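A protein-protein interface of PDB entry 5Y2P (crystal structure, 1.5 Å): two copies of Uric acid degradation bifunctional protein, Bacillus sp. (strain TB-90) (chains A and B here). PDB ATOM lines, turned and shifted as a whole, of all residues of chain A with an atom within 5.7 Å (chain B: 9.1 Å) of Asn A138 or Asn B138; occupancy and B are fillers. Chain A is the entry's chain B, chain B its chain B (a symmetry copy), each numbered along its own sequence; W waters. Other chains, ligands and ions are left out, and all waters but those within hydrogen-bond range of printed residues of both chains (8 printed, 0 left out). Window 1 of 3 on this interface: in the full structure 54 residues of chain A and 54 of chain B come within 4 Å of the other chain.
N of Lys A135 sits at hydrogen-bond distance from O of Gln B168.
NZ of Lys A134 is in salt-bridge range of OE2 of Glu B139 (2.7 Å).
The side-chain hydroxyl of Ser A136 is in hydrogen-bond range of the side-chain amide nitrogen of Asn B138, 3.3 Å away.
The backbone NH (N) of Arg A137 is in hydrogen-bond range of the side-chain amide oxygen (OD1) of Asn B138 (2.7 Å).
The guanidinium group of Arg A137 lies within hydrogen-bond range of the backbone carbonyl oxygen of Gly B166.
The backbone carbonyl oxygen (O) of Gly A166 is in hydrogen-bond range of the guanidinium group (NH2) of Arg B137 (2.8 Å).
The backbone NH (N) of Arg B137 is in hydrogen-bond range of the side-chain amide oxygen (OD1) of Asn A138, at 2.7 Å.
The side-chain amide nitrogen of Asn A138 lies close to the side-chain amide nitrogen of Asn B138, at 3.1 Å.
OE2 of Glu A139 is in salt-bridge range of NZ of Lys B134 (2.7 Å).
The side-chain amide nitrogen (ND2) of Asn A138 sits at hydrogen-bond distance from the side-chain hydroxyl (OG) of Ser B136 (3.3 Å).
The side-chain hydroxyl (OG) of Ser A136 lies within hydrogen-bond range of the backbone NH (N) of Asn A138.
The side-chain amino group of Lys A134 lies within salt-bridge range of the side-chain carboxylate of Glu A116.
The backbone carbonyl oxygen of Pro A114 lies within hydrogen-bond range of the backbone NH of Ser A136.
The backbone carbonyl oxygen (O) of Lys B135 sits at hydrogen-bond distance from the guanidinium group (NH1) of Arg B137 (3.2 Å).
The side-chain carboxylate of Glu B116 is in salt-bridge range of the side-chain amino group of Lys B134 (3.6 Å).
OG of Ser B136 sits at hydrogen-bond distance from N of Asn B138, at 3.1 Å.
Gln B168 touches Lys A134.
Lys A135 touches Asn B138.
O of Arg B137 touches NH2 of Arg A137 (3.5 Å).
Arg A137 touches Gln B168.
Asn A138 touches Lys B135.
Printed residues of chain A that touch a printed residue of chain B: Lys A134, Lys A135, Ser A136, Arg A137, Asn A138, Glu A139 and Gly A166.
Among the printed residues, 15 pairs touch across the chains.
Among the printed residues, Asp or Glu carboxylates within 4 Å of a Lys or Arg side-chain nitrogen of the other chain: Lys A134 with Glu B139 (2.7 Å) and Glu A139 with Lys B134 (2.7 Å).
Lys A134 touches Glu B139, and with the chains exchanged Glu A139 touches Lys B134.
Arg A137 touches Asn B138, and with the chains exchanged Asn A138 touches Arg B137.
Arg A137 touches Gly B166, and with the chains exchanged Gly A166 touches Arg B137.
Asn A138 touches its own counterpart, Asn B138.
Of the 15 pairs that touch across the chains among the printed residues, 12 have their exchanged pair printed and touching as well.
Water W5 lies within hydrogen-bond range of OE2 of Glu A116 (2.7 Å), OE1 of Glu B116 (2.7 Å), NZ of Lys B134 (2.9 Å) and ND2 of Asn A138 (2.9 Å).
Water W2 lies within hydrogen-bond range of OE2 of Glu B116, OE1 of Glu A116, NZ of Lys A134 and ND2 of Asn B138.
Water W7 bridges the backbone carbonyl oxygen of Arg A137 and the guanidinium group of Arg B137.
Water W6 bridges O of Arg B137 (2.7 Å) and NE of Arg A137 (3.0 Å).
Water W3 lies within hydrogen-bond range of O of Asn A138, NH2 of Arg B137 and O of Arg A137.
Water W8 lies within hydrogen-bond range of the backbone carbonyl oxygen of Asn B138 (2.9 Å), the guanidinium group of Arg A137 (3.1 Å) and the backbone carbonyl oxygen of Arg B137 (3.2 Å).
Of the printed residues of chain B, Asn A138 touches Lys B135, Ser B136, Arg B137 and Asn B138.
Of the printed residues of chain A, Asn B138 touches Lys A135 (3.8 Å), Ser A136 (3.3 Å), Arg A137 (2.7 Å) and Asn A138 (3.1 Å).
Ser A136 touches one residue of chain B.
Arg A137 touches four residues of chain B.
Glu A139 touches just one residue of chain B: Lys B134.
Of the printed residues of chain A, Glu B139 touches Lys A134.
Of the printed residues of chain A, Gln B168 touches Lys A134, Lys A135 and Arg A137.
Of the printed residues of chain A, Lys B134 touches Glu A139.
Of the printed residues of chain B, Lys A134 touches Glu B139 and Gln B168.
Printed residues of chain B within 4 Å of Lys A135: Asn B138 (3.8 Å) and Gln B168 (3.0 Å).
Glu B116 touches none of the printed residues of chain A.
Pro B114 touches none of the printed residues of chain A.
The nearest printed residue of chain A that does not touch Asn B138 is Glu A116 (4.3 Å).
The nearest printed residue of chain A that does not touch Gln B168 is Ser A136 (5.9 Å).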
ATOM      1  N   PRO A 114      -5.315 -17.767 -36.226  1.00  0.00           N
ATOM      2  CA  PRO A 114      -6.486 -16.955 -36.559  1.00  0.00           C
ATOM      3  C   PRO A 114      -6.235 -15.460 -36.499  1.00  0.00           C
ATOM      4  O   PRO A 114      -5.481 -14.957 -35.657  1.00  0.00           O
ATOM      5  CB  PRO A 114      -7.519 -17.373 -35.493  1.00  0.00           C
ATOM      6  CG  PRO A 114      -6.704 -17.704 -34.285  1.00  0.00           C
ATOM      7  CD  PRO A 114      -5.385 -18.293 -34.844  1.00  0.00           C
ATOM      8  N   GLU A 116      -8.545 -11.663 -36.800  1.00  0.00           N
ATOM      9  CA  GLU A 116      -9.859 -11.060 -36.696  1.00  0.00           C
ATOM     10  C   GLU A 116      -9.905  -9.746 -37.451  1.00  0.00           C
ATOM     11  O   GLU A 116      -8.885  -9.114 -37.699  1.00  0.00           O
ATOM     12  CB  GLU A 116     -10.235 -10.846 -35.228  1.00  0.00           C
ATOM     13  CG  GLU A 116     -10.454 -12.155 -34.520  1.00  0.00           C
ATOM     14  CD  GLU A 116     -10.711 -12.068 -33.024  1.00  0.00           C
ATOM     15  OE1 GLU A 116     -10.725 -10.980 -32.446  1.00  0.00           O
ATOM     16  OE2 GLU A 116     -10.899 -13.157 -32.462  1.00  0.00           O
ATOM     17  N   LYS A 134      -6.212  -8.404 -37.006  1.00  0.00           N
ATOM     18  CA  LYS A 134      -5.715  -8.505 -35.644  1.00  0.00           C
ATOM     19  C   LYS A 134      -5.386  -9.968 -35.370  1.00  0.00           C
ATOM     20  O   LYS A 134      -6.258 -10.830 -35.529  1.00  0.00           O
ATOM     21  CB  LYS A 134      -6.813  -8.007 -34.699  1.00  0.00           C
ATOM     22  CG  LYS A 134      -6.411  -7.867 -33.275  1.00  0.00           C
ATOM     23  CD  LYS A 134      -7.574  -7.280 -32.492  1.00  0.00           C
ATOM     24  CE  LYS A 134      -8.467  -8.400 -31.947  1.00  0.00           C
ATOM     25  NZ  LYS A 134      -9.538  -7.860 -31.038  1.00  0.00           N
ATOM     26  N   LYS A 135      -4.153 -10.217 -34.948  1.00  0.00           N
ATOM     27  CA  LYS A 135      -3.773 -11.560 -34.547  1.00  0.00           C
ATOM     28  C   LYS A 135      -4.558 -11.956 -33.307  1.00  0.00           C
ATOM     29  O   LYS A 135      -4.666 -11.187 -32.340  1.00  0.00           O
ATOM     30  CB  LYS A 135      -2.288 -11.624 -34.252  1.00  0.00           C
ATOM     31  CG  LYS A 135      -1.827 -13.038 -33.903  1.00  0.00           C
ATOM     32  CD  LYS A 135      -0.328 -13.146 -34.108  1.00  0.00           C
ATOM     33  CE  LYS A 135       0.126 -14.485 -34.623  1.00  0.00           C
ATOM     34  NZ  LYS A 135      -0.228 -15.529 -33.685  1.00  0.00           N
ATOM     35  N   SER A 136      -5.135 -13.146 -33.340  1.00  0.00           N
ATOM     36  CA  SER A 136      -5.843 -13.659 -32.173  1.00  0.00           C
ATOM     37  C   SER A 136      -5.069 -14.796 -31.523  1.00  0.00           C
ATOM     38  O   SER A 136      -4.666 -15.761 -32.191  1.00  0.00           O
ATOM     39  CB  SER A 136      -7.258 -14.139 -32.498  1.00  0.00           C
ATOM     40  OG  SER A 136      -7.875 -14.670 -31.322  1.00  0.00           O
ATOM     41  N   ARG A 137      -4.935 -14.701 -30.202  1.00  0.00           N
ATOM     42  CA  ARG A 137      -4.336 -15.743 -29.385  1.00  0.00           C
ATOM     43  C   ARG A 137      -5.415 -16.505 -28.621  1.00  0.00           C
ATOM     44  O   ARG A 137      -5.126 -17.152 -27.614  1.00  0.00           O
ATOM     45  CB  ARG A 137      -3.321 -15.118 -28.442  1.00  0.00           C
ATOM     46  CG  ARG A 137      -2.097 -14.566 -29.185  1.00  0.00           C
ATOM     47  CD  ARG A 137      -2.267 -13.135 -29.671  1.00  0.00           C
ATOM     48  NE  ARG A 137      -2.114 -12.173 -28.603  1.00  0.00           N
ATOM     49  CZ  ARG A 137      -2.429 -10.881 -28.680  1.00  0.00           C
ATOM     50  NH1 ARG A 137      -2.958 -10.390 -29.794  1.00  0.00           N
ATOM     51  NH2 ARG A 137      -2.235 -10.081 -27.660  1.00  0.00           N
ATOM     52  N   ASN A 138      -6.652 -16.440 -29.099  1.00  0.00           N
ATOM     53  CA  ASN A 138      -7.724 -17.203 -28.476  1.00  0.00           C
ATOM     54  C   ASN A 138      -7.909 -18.547 -29.186  1.00  0.00           C
ATOM     55  O   ASN A 138      -6.917 -19.175 -29.585  1.00  0.00           O
ATOM     56  CB  ASN A 138      -8.990 -16.356 -28.391  1.00  0.00           C
ATOM     57  CG  ASN A 138      -8.776 -15.126 -27.583  1.00  0.00           C
ATOM     58  OD1 ASN A 138      -7.991 -15.153 -26.642  1.00  0.00           O
ATOM     59  ND2 ASN A 138      -9.476 -14.068 -27.881  1.00  0.00           N
ATOM     60  N   GLU A 139      -9.150 -19.024 -29.336  1.00  0.00           N
ATOM     61  CA  GLU A 139      -9.375 -20.364 -29.863  1.00  0.00           C
ATOM     62  C   GLU A 139      -9.008 -20.435 -31.340  1.00  0.00           C
ATOM     63  O   GLU A 139      -8.963 -19.419 -32.046  1.00  0.00           O
ATOM     64  CB  GLU A 139     -10.824 -20.826 -29.626  1.00  0.00           C
ATOM     65  CG  GLU A 139     -11.909 -20.064 -30.356  1.00  0.00           C
ATOM     66  CD  GLU A 139     -12.311 -18.757 -29.720  1.00  0.00           C
ATOM     67  OE1 GLU A 139     -11.730 -18.282 -28.713  1.00  0.00           O
ATOM     68  OE2 GLU A 139     -13.292 -18.163 -30.257  1.00  0.00           O
ATOM     69  N   TYR A 140      -8.705 -21.649 -31.794  1.00  0.00           N
ATOM     70  CA  TYR A 140      -8.235 -21.851 -33.161  1.00  0.00           C
ATOM     71  C   TYR A 140      -8.652 -23.232 -33.657  1.00  0.00           C
ATOM     72  O   TYR A 140      -8.768 -24.184 -32.883  1.00  0.00           O
ATOM     73  CB  TYR A 140      -6.709 -21.658 -33.253  1.00  0.00           C
ATOM     74  CG  TYR A 140      -5.913 -22.528 -32.324  1.00  0.00           C
ATOM     75  CD1 TYR A 140      -5.679 -22.149 -31.002  1.00  0.00           C
ATOM     76  CD2 TYR A 140      -5.391 -23.745 -32.751  1.00  0.00           C
ATOM     77  CE1 TYR A 140      -4.949 -22.942 -30.146  1.00  0.00           C
ATOM     78  CE2 TYR A 140      -4.653 -24.534 -31.897  1.00  0.00           C
ATOM     79  CZ  TYR A 140      -4.453 -24.132 -30.597  1.00  0.00           C
ATOM     80  OH  TYR A 140      -3.724 -24.909 -29.710  1.00  0.00           O
ATOM     81  N   ALA A 165      -9.507 -25.806 -30.621  1.00  0.00           N
ATOM     82  CA  ALA A 165      -8.647 -25.806 -29.453  1.00  0.00           C
ATOM     83  C   ALA A 165      -8.633 -24.431 -28.809  1.00  0.00           C
ATOM     84  O   ALA A 165      -8.854 -23.416 -29.467  1.00  0.00           O
ATOM     85  CB  ALA A 165      -7.198 -26.151 -29.884  1.00  0.00           C
ATOM     86  N   GLY A 166      -8.371 -24.387 -27.503  1.00  0.00           N
ATOM     87  CA  GLY A 166      -8.151 -23.122 -26.822  1.00  0.00           C
ATOM     88  C   GLY A 166      -9.396 -22.317 -26.533  1.00  0.00           C
ATOM     89  O   GLY A 166      -9.287 -21.098 -26.314  1.00  0.00           O
ATOM     90  N   GLU B 112      -6.734  -4.834 -17.272  1.00  0.00           N
ATOM     91  CA  GLU B 112      -7.991  -5.502 -17.565  1.00  0.00           C
ATOM     92  C   GLU B 112      -7.742  -6.956 -17.916  1.00  0.00           C
ATOM     93  O   GLU B 112      -6.762  -7.296 -18.603  1.00  0.00           O
ATOM     94  CB  GLU B 112      -8.645  -4.846 -18.773  1.00  0.00           C
ATOM     95  CG  GLU B 112      -9.924  -5.523 -19.274  1.00  0.00           C
ATOM     96  CD  GLU B 112     -10.415  -4.947 -20.582  1.00  0.00           C
ATOM     97  OE1 GLU B 112      -9.617  -4.538 -21.451  1.00  0.00           O
ATOM     98  OE2 GLU B 112     -11.660  -4.947 -20.781  1.00  0.00           O
ATOM     99  N   ILE B 113      -8.641  -7.817 -17.448  1.00  0.00           N
ATOM    100  CA  ILE B 113      -8.708  -9.202 -17.896  1.00  0.00           C
ATOM    101  C   ILE B 113      -9.966  -9.235 -18.752  1.00  0.00           C
ATOM    102  O   ILE B 113     -11.081  -9.246 -18.209  1.00  0.00           O
ATOM    103  CB  ILE B 113      -8.750 -10.176 -16.710  1.00  0.00           C
ATOM    104  CG1 ILE B 113      -7.551  -9.931 -15.777  1.00  0.00           C
ATOM    105  CG2 ILE B 113      -8.782 -11.613 -17.236  1.00  0.00           C
ATOM    106  CD1 ILE B 113      -7.773 -10.421 -14.381  1.00  0.00           C
ATOM    107  N   PRO B 114      -9.842  -9.166 -20.074  1.00  0.00           N
ATOM    108  CA  PRO B 114     -11.013  -8.975 -20.932  1.00  0.00           C
ATOM    109  C   PRO B 114     -11.762 -10.257 -21.246  1.00  0.00           C
ATOM    110  O   PRO B 114     -11.175 -11.335 -21.406  1.00  0.00           O
ATOM    111  CB  PRO B 114     -10.412  -8.372 -22.218  1.00  0.00           C
ATOM    112  CG  PRO B 114      -9.048  -8.974 -22.318  1.00  0.00           C
ATOM    113  CD  PRO B 114      -8.582  -9.151 -20.851  1.00  0.00           C
ATOM    114  N   PHE B 115     -13.086 -10.111 -21.337  1.00  0.00           N
ATOM    115  CA  PHE B 115     -13.982 -11.179 -21.739  1.00  0.00           C
ATOM    116  C   PHE B 115     -14.858 -10.720 -22.897  1.00  0.00           C
ATOM    117  O   PHE B 115     -15.298  -9.567 -22.938  1.00  0.00           O
ATOM    118  CB  PHE B 115     -14.873 -11.638 -20.574  1.00  0.00           C
ATOM    119  CG  PHE B 115     -14.087 -12.213 -19.413  1.00  0.00           C
ATOM    120  CD1 PHE B 115     -13.540 -11.389 -18.460  1.00  0.00           C
ATOM    121  CD2 PHE B 115     -13.813 -13.565 -19.355  1.00  0.00           C
ATOM    122  CE1 PHE B 115     -12.780 -11.910 -17.416  1.00  0.00           C
ATOM    123  CE2 PHE B 115     -13.042 -14.094 -18.318  1.00  0.00           C
ATOM    124  CZ  PHE B 115     -12.531 -13.270 -17.358  1.00  0.00           C
ATOM    125  N   GLU B 116     -15.124 -11.623 -23.829  1.00  0.00           N
ATOM    126  CA  GLU B 116     -15.917 -11.322 -25.005  1.00  0.00           C
ATOM    127  C   GLU B 116     -17.248 -12.046 -24.950  1.00  0.00           C
ATOM    128  O   GLU B 116     -17.404 -13.049 -24.262  1.00  0.00           O
ATOM    129  CB  GLU B 116     -15.154 -11.702 -26.276  1.00  0.00           C
ATOM    130  CG  GLU B 116     -13.962 -10.811 -26.489  1.00  0.00           C
ATOM    131  CD  GLU B 116     -13.058 -11.174 -27.656  1.00  0.00           C
ATOM    132  OE1 GLU B 116     -13.303 -12.152 -28.365  1.00  0.00           O
ATOM    133  OE2 GLU B 116     -12.087 -10.421 -27.820  1.00  0.00           O
ATOM    134  N   LYS B 134     -16.304 -15.376 -23.036  1.00  0.00           N
ATOM    135  CA  LYS B 134     -15.091 -16.007 -23.529  1.00  0.00           C
ATOM    136  C   LYS B 134     -13.902 -15.195 -23.031  1.00  0.00           C
ATOM    137  O   LYS B 134     -13.839 -13.987 -23.283  1.00  0.00           O
ATOM    138  CB  LYS B 134     -15.146 -16.012 -25.060  1.00  0.00           C
ATOM    139  CG  LYS B 134     -14.069 -16.785 -25.733  1.00  0.00           C
ATOM    140  CD  LYS B 134     -14.315 -16.768 -27.231  1.00  0.00           C
ATOM    141  CE  LYS B 134     -13.611 -15.568 -27.873  1.00  0.00           C
ATOM    142  NZ  LYS B 134     -13.705 -15.609 -29.374  1.00  0.00           N
ATOM    143  N   LYS B 135     -12.979 -15.871 -22.356  1.00  0.00           N
ATOM    144  CA  LYS B 135     -11.751 -15.216 -21.940  1.00  0.00           C
ATOM    145  C   LYS B 135     -10.945 -14.830 -23.169  1.00  0.00           C
ATOM    146  O   LYS B 135     -10.762 -15.631 -24.098  1.00  0.00           O
ATOM    147  CB  LYS B 135     -10.931 -16.140 -21.063  1.00  0.00           C
ATOM    148  CG  LYS B 135      -9.667 -15.466 -20.534  1.00  0.00           C
ATOM    149  CD  LYS B 135      -9.167 -16.214 -19.313  1.00  0.00           C
ATOM    150  CE  LYS B 135      -8.559 -15.331 -18.258  1.00  0.00           C
ATOM    151  NZ  LYS B 135      -7.414 -14.626 -18.794  1.00  0.00           N
ATOM    152  N   SER B 136     -10.484 -13.590 -23.195  1.00  0.00           N
ATOM    153  CA  SER B 136      -9.630 -13.139 -24.288  1.00  0.00           C
ATOM    154  C   SER B 136      -8.197 -12.948 -23.815  1.00  0.00           C
ATOM    155  O   SER B 136      -7.938 -12.266 -22.811  1.00  0.00           O
ATOM    156  CB  SER B 136     -10.121 -11.842 -24.933  1.00  0.00           C
ATOM    157  OG  SER B 136      -9.215 -11.435 -25.960  1.00  0.00           O
ATOM    158  N   ARG B 137      -7.270 -13.498 -24.597  1.00  0.00           N
ATOM    159  CA  ARG B 137      -5.842 -13.325 -24.384  1.00  0.00           C
ATOM    160  C   ARG B 137      -5.268 -12.346 -25.404  1.00  0.00           C
ATOM    161  O   ARG B 137      -4.061 -12.340 -25.651  1.00  0.00           O
ATOM    162  CB  ARG B 137      -5.157 -14.678 -24.462  1.00  0.00           C
ATOM    163  CG  ARG B 137      -5.535 -15.592 -23.288  1.00  0.00           C
ATOM    164  CD  ARG B 137      -6.794 -16.411 -23.529  1.00  0.00           C
ATOM    165  NE  ARG B 137      -6.554 -17.542 -24.397  1.00  0.00           N
ATOM    166  CZ  ARG B 137      -7.498 -18.294 -24.961  1.00  0.00           C
ATOM    167  NH1 ARG B 137      -8.779 -18.009 -24.768  1.00  0.00           N
ATOM    168  NH2 ARG B 137      -7.179 -19.314 -25.720  1.00  0.00           N
ATOM    169  N   ASN B 138      -6.122 -11.515 -25.990  1.00  0.00           N
ATOM    170  CA  ASN B 138      -5.644 -10.498 -26.914  1.00  0.00           C
ATOM    171  C   ASN B 138      -5.418  -9.171 -26.183  1.00  0.00           C
ATOM    172  O   ASN B 138      -4.942  -9.172 -25.038  1.00  0.00           O
ATOM    173  CB  ASN B 138      -6.577 -10.402 -28.118  1.00  0.00           C
ATOM    174  CG  ASN B 138      -6.656 -11.690 -28.857  1.00  0.00           C
ATOM    175  OD1 ASN B 138      -5.673 -12.421 -28.898  1.00  0.00           O
ATOM    176  ND2 ASN B 138      -7.765 -11.972 -29.479  1.00  0.00           N
ATOM    177  N   GLU B 139      -5.719  -8.033 -26.818  1.00  0.00           N
ATOM    178  CA  GLU B 139      -5.382  -6.741 -26.234  1.00  0.00           C
ATOM    179  C   GLU B 139      -6.240  -6.460 -25.006  1.00  0.00           C
ATOM    180  O   GLU B 139      -7.324  -7.030 -24.828  1.00  0.00           O
ATOM    181  CB  GLU B 139      -5.501  -5.608 -27.268  1.00  0.00           C
ATOM    182  CG  GLU B 139      -6.888  -5.310 -27.795  1.00  0.00           C
ATOM    183  CD  GLU B 139      -7.372  -6.237 -28.882  1.00  0.00           C
ATOM    184  OE1 GLU B 139      -6.719  -7.241 -29.261  1.00  0.00           O
ATOM    185  OE2 GLU B 139      -8.483  -5.935 -29.408  1.00  0.00           O
ATOM    186  N   TYR B 140      -5.721  -5.598 -24.134  1.00  0.00           N
ATOM    187  CA  TYR B 140      -6.383  -5.313 -22.865  1.00  0.00           C
ATOM    188  C   TYR B 140      -6.074  -3.887 -22.424  1.00  0.00           C
ATOM    189  O   TYR B 140      -5.007  -3.342 -22.715  1.00  0.00           O
ATOM    190  CB  TYR B 140      -5.973  -6.337 -21.788  1.00  0.00           C
ATOM    191  CG  TYR B 140      -4.493  -6.442 -21.561  1.00  0.00           C
ATOM    192  CD1 TYR B 140      -3.695  -7.263 -22.358  1.00  0.00           C
ATOM    193  CD2 TYR B 140      -3.868  -5.716 -20.550  1.00  0.00           C
ATOM    194  CE1 TYR B 140      -2.338  -7.365 -22.152  1.00  0.00           C
ATOM    195  CE2 TYR B 140      -2.512  -5.825 -20.339  1.00  0.00           C
ATOM    196  CZ  TYR B 140      -1.757  -6.636 -21.153  1.00  0.00           C
ATOM    197  OH  TYR B 140      -0.388  -6.758 -20.974  1.00  0.00           O
ATOM    198  N   ALA B 141      -7.012  -3.288 -21.700  1.00  0.00           N
ATOM    199  CA  ALA B 141      -6.815  -1.958 -21.157  1.00  0.00           C
ATOM    200  C   ALA B 141      -5.929  -1.998 -19.916  1.00  0.00           C
ATOM    201  O   ALA B 141      -5.867  -2.996 -19.185  1.00  0.00           O
ATOM    202  CB  ALA B 141      -8.171  -1.363 -20.775  1.00  0.00           C
ATOM    203  N   LEU B 164      -3.563   0.855 -23.522  1.00  0.00           N
ATOM    204  CA  LEU B 164      -3.981  -0.312 -24.262  1.00  0.00           C
ATOM    205  C   LEU B 164      -2.735  -1.119 -24.573  1.00  0.00           C
ATOM    206  O   LEU B 164      -1.782  -0.596 -25.166  1.00  0.00           O
ATOM    207  CB  LEU B 164      -4.641   0.112 -25.583  1.00  0.00           C
ATOM    208  CG  LEU B 164      -5.064  -1.040 -26.503  1.00  0.00           C
ATOM    209  CD1 LEU B 164      -6.257  -1.802 -25.965  1.00  0.00           C
ATOM    210  CD2 LEU B 164      -5.348  -0.436 -27.887  1.00  0.00           C
ATOM    211  N   ALA B 165      -2.733  -2.378 -24.196  1.00  0.00           N
ATOM    212  CA  ALA B 165      -1.578  -3.242 -24.339  1.00  0.00           C
ATOM    213  C   ALA B 165      -1.935  -4.470 -25.157  1.00  0.00           C
ATOM    214  O   ALA B 165      -3.088  -4.895 -25.198  1.00  0.00           O
ATOM    215  CB  ALA B 165      -1.115  -3.716 -22.936  1.00  0.00           C
ATOM    216  N   GLY B 166      -0.939  -5.052 -25.824  1.00  0.00           N
ATOM    217  CA  GLY B 166      -1.125  -6.332 -26.487  1.00  0.00           C
ATOM    218  C   GLY B 166      -1.881  -6.279 -27.794  1.00  0.00           C
ATOM    219  O   GLY B 166      -2.410  -7.319 -28.226  1.00  0.00           O
ATOM    220  N   LEU B 167      -1.928  -5.127 -28.451  1.00  0.00           N
ATOM    221  CA  LEU B 167      -2.559  -5.032 -29.754  1.00  0.00           C
ATOM    222  C   LEU B 167      -1.567  -5.521 -30.810  1.00  0.00           C
ATOM    223  O   LEU B 167      -0.411  -5.095 -30.831  1.00  0.00           O
ATOM    224  CB  LEU B 167      -2.979  -3.599 -30.042  1.00  0.00           C
ATOM    225  CG  LEU B 167      -3.842  -3.351 -31.295  1.00  0.00           C
ATOM    226  CD1 LEU B 167      -5.150  -4.143 -31.215  1.00  0.00           C
ATOM    227  CD2 LEU B 167      -4.140  -1.870 -31.435  1.00  0.00           C
ATOM    228  N   GLN B 168      -1.997  -6.469 -31.624  1.00  0.00           N
ATOM    229  CA  GLN B 168      -1.160  -7.079 -32.651  1.00  0.00           C
ATOM    230  C   GLN B 168      -1.862  -6.975 -33.996  1.00  0.00           C
ATOM    231  O   GLN B 168      -2.876  -7.633 -34.216  1.00  0.00           O
ATOM    232  CB  GLN B 168      -0.870  -8.538 -32.312  1.00  0.00           C
ATOM    233  CG  GLN B 168      -0.160  -8.750 -30.966  1.00  0.00           C
ATOM    234  CD  GLN B 168       0.258 -10.167 -30.746  1.00  0.00           C
ATOM    235  OE1 GLN B 168       0.075 -11.052 -31.590  1.00  0.00           O
ATOM    236  NE2 GLN B 168       0.883 -10.404 -29.602  1.00  0.00           N
ATOM    237  N   LEU B 200       1.542  -3.166 -30.679  1.00  0.00           N
ATOM    238  CA  LEU B 200       1.401  -1.818 -30.152  1.00  0.00           C
ATOM    239  C   LEU B 200       0.979  -1.845 -28.696  1.00  0.00           C
ATOM    240  O   LEU B 200       0.027  -2.538 -28.334  1.00  0.00           O
ATOM    241  CB  LEU B 200       0.343  -1.051 -30.929  1.00  0.00           C
ATOM    242  CG  LEU B 200       0.651  -0.776 -32.396  1.00  0.00           C
ATOM    243  CD1 LEU B 200      -0.564  -0.136 -33.022  1.00  0.00           C
ATOM    244  CD2 LEU B 200       1.847   0.156 -32.555  1.00  0.00           C
ATOM    245  N   ARG B 227      -8.024   1.682 -29.644  1.00  0.00           N
ATOM    246  CA  ARG B 227      -7.807   0.544 -30.529  1.00  0.00           C
ATOM    247  C   ARG B 227      -8.336   0.849 -31.929  1.00  0.00           C
ATOM    248  O   ARG B 227      -7.679   0.561 -32.941  1.00  0.00           O
ATOM    249  CB  ARG B 227      -8.513  -0.697 -29.990  1.00  0.00           C
ATOM    250  CG  ARG B 227      -8.367  -1.837 -31.002  1.00  0.00           C
ATOM    251  CD  ARG B 227      -9.200  -3.001 -30.777  1.00  0.00           C
ATOM    252  NE  ARG B 227     -10.572  -2.660 -30.406  1.00  0.00           N
ATOM    253  CZ  ARG B 227     -11.194  -3.191 -29.373  1.00  0.00           C
ATOM    254  NH1 ARG B 227     -10.596  -4.111 -28.627  1.00  0.00           N
ATOM    255  NH2 ARG B 227     -12.430  -2.821 -29.094  1.00  0.00           N
HETATM  256  O   HOH W   1      -4.368  -8.023 -30.722  1.00  0.00           O
HETATM  257  O   HOH W   2     -10.245 -10.428 -29.800  1.00  0.00           O
HETATM  258  O   HOH W   3      -5.100 -20.362 -27.697  1.00  0.00           O
HETATM  259  O   HOH W   4     -11.386 -18.655 -25.882  1.00  0.00           O
HETATM  260  O   HOH W   5     -11.579 -13.649 -29.890  1.00  0.00           O
HETATM  261  O   HOH W   6      -1.517 -13.256 -25.842  1.00  0.00           O
HETATM  262  O   HOH W   7      -3.732 -17.924 -25.419  1.00  0.00           O
HETATM  263  O   HOH W   8      -2.203  -9.938 -24.609  1.00  0.00           O
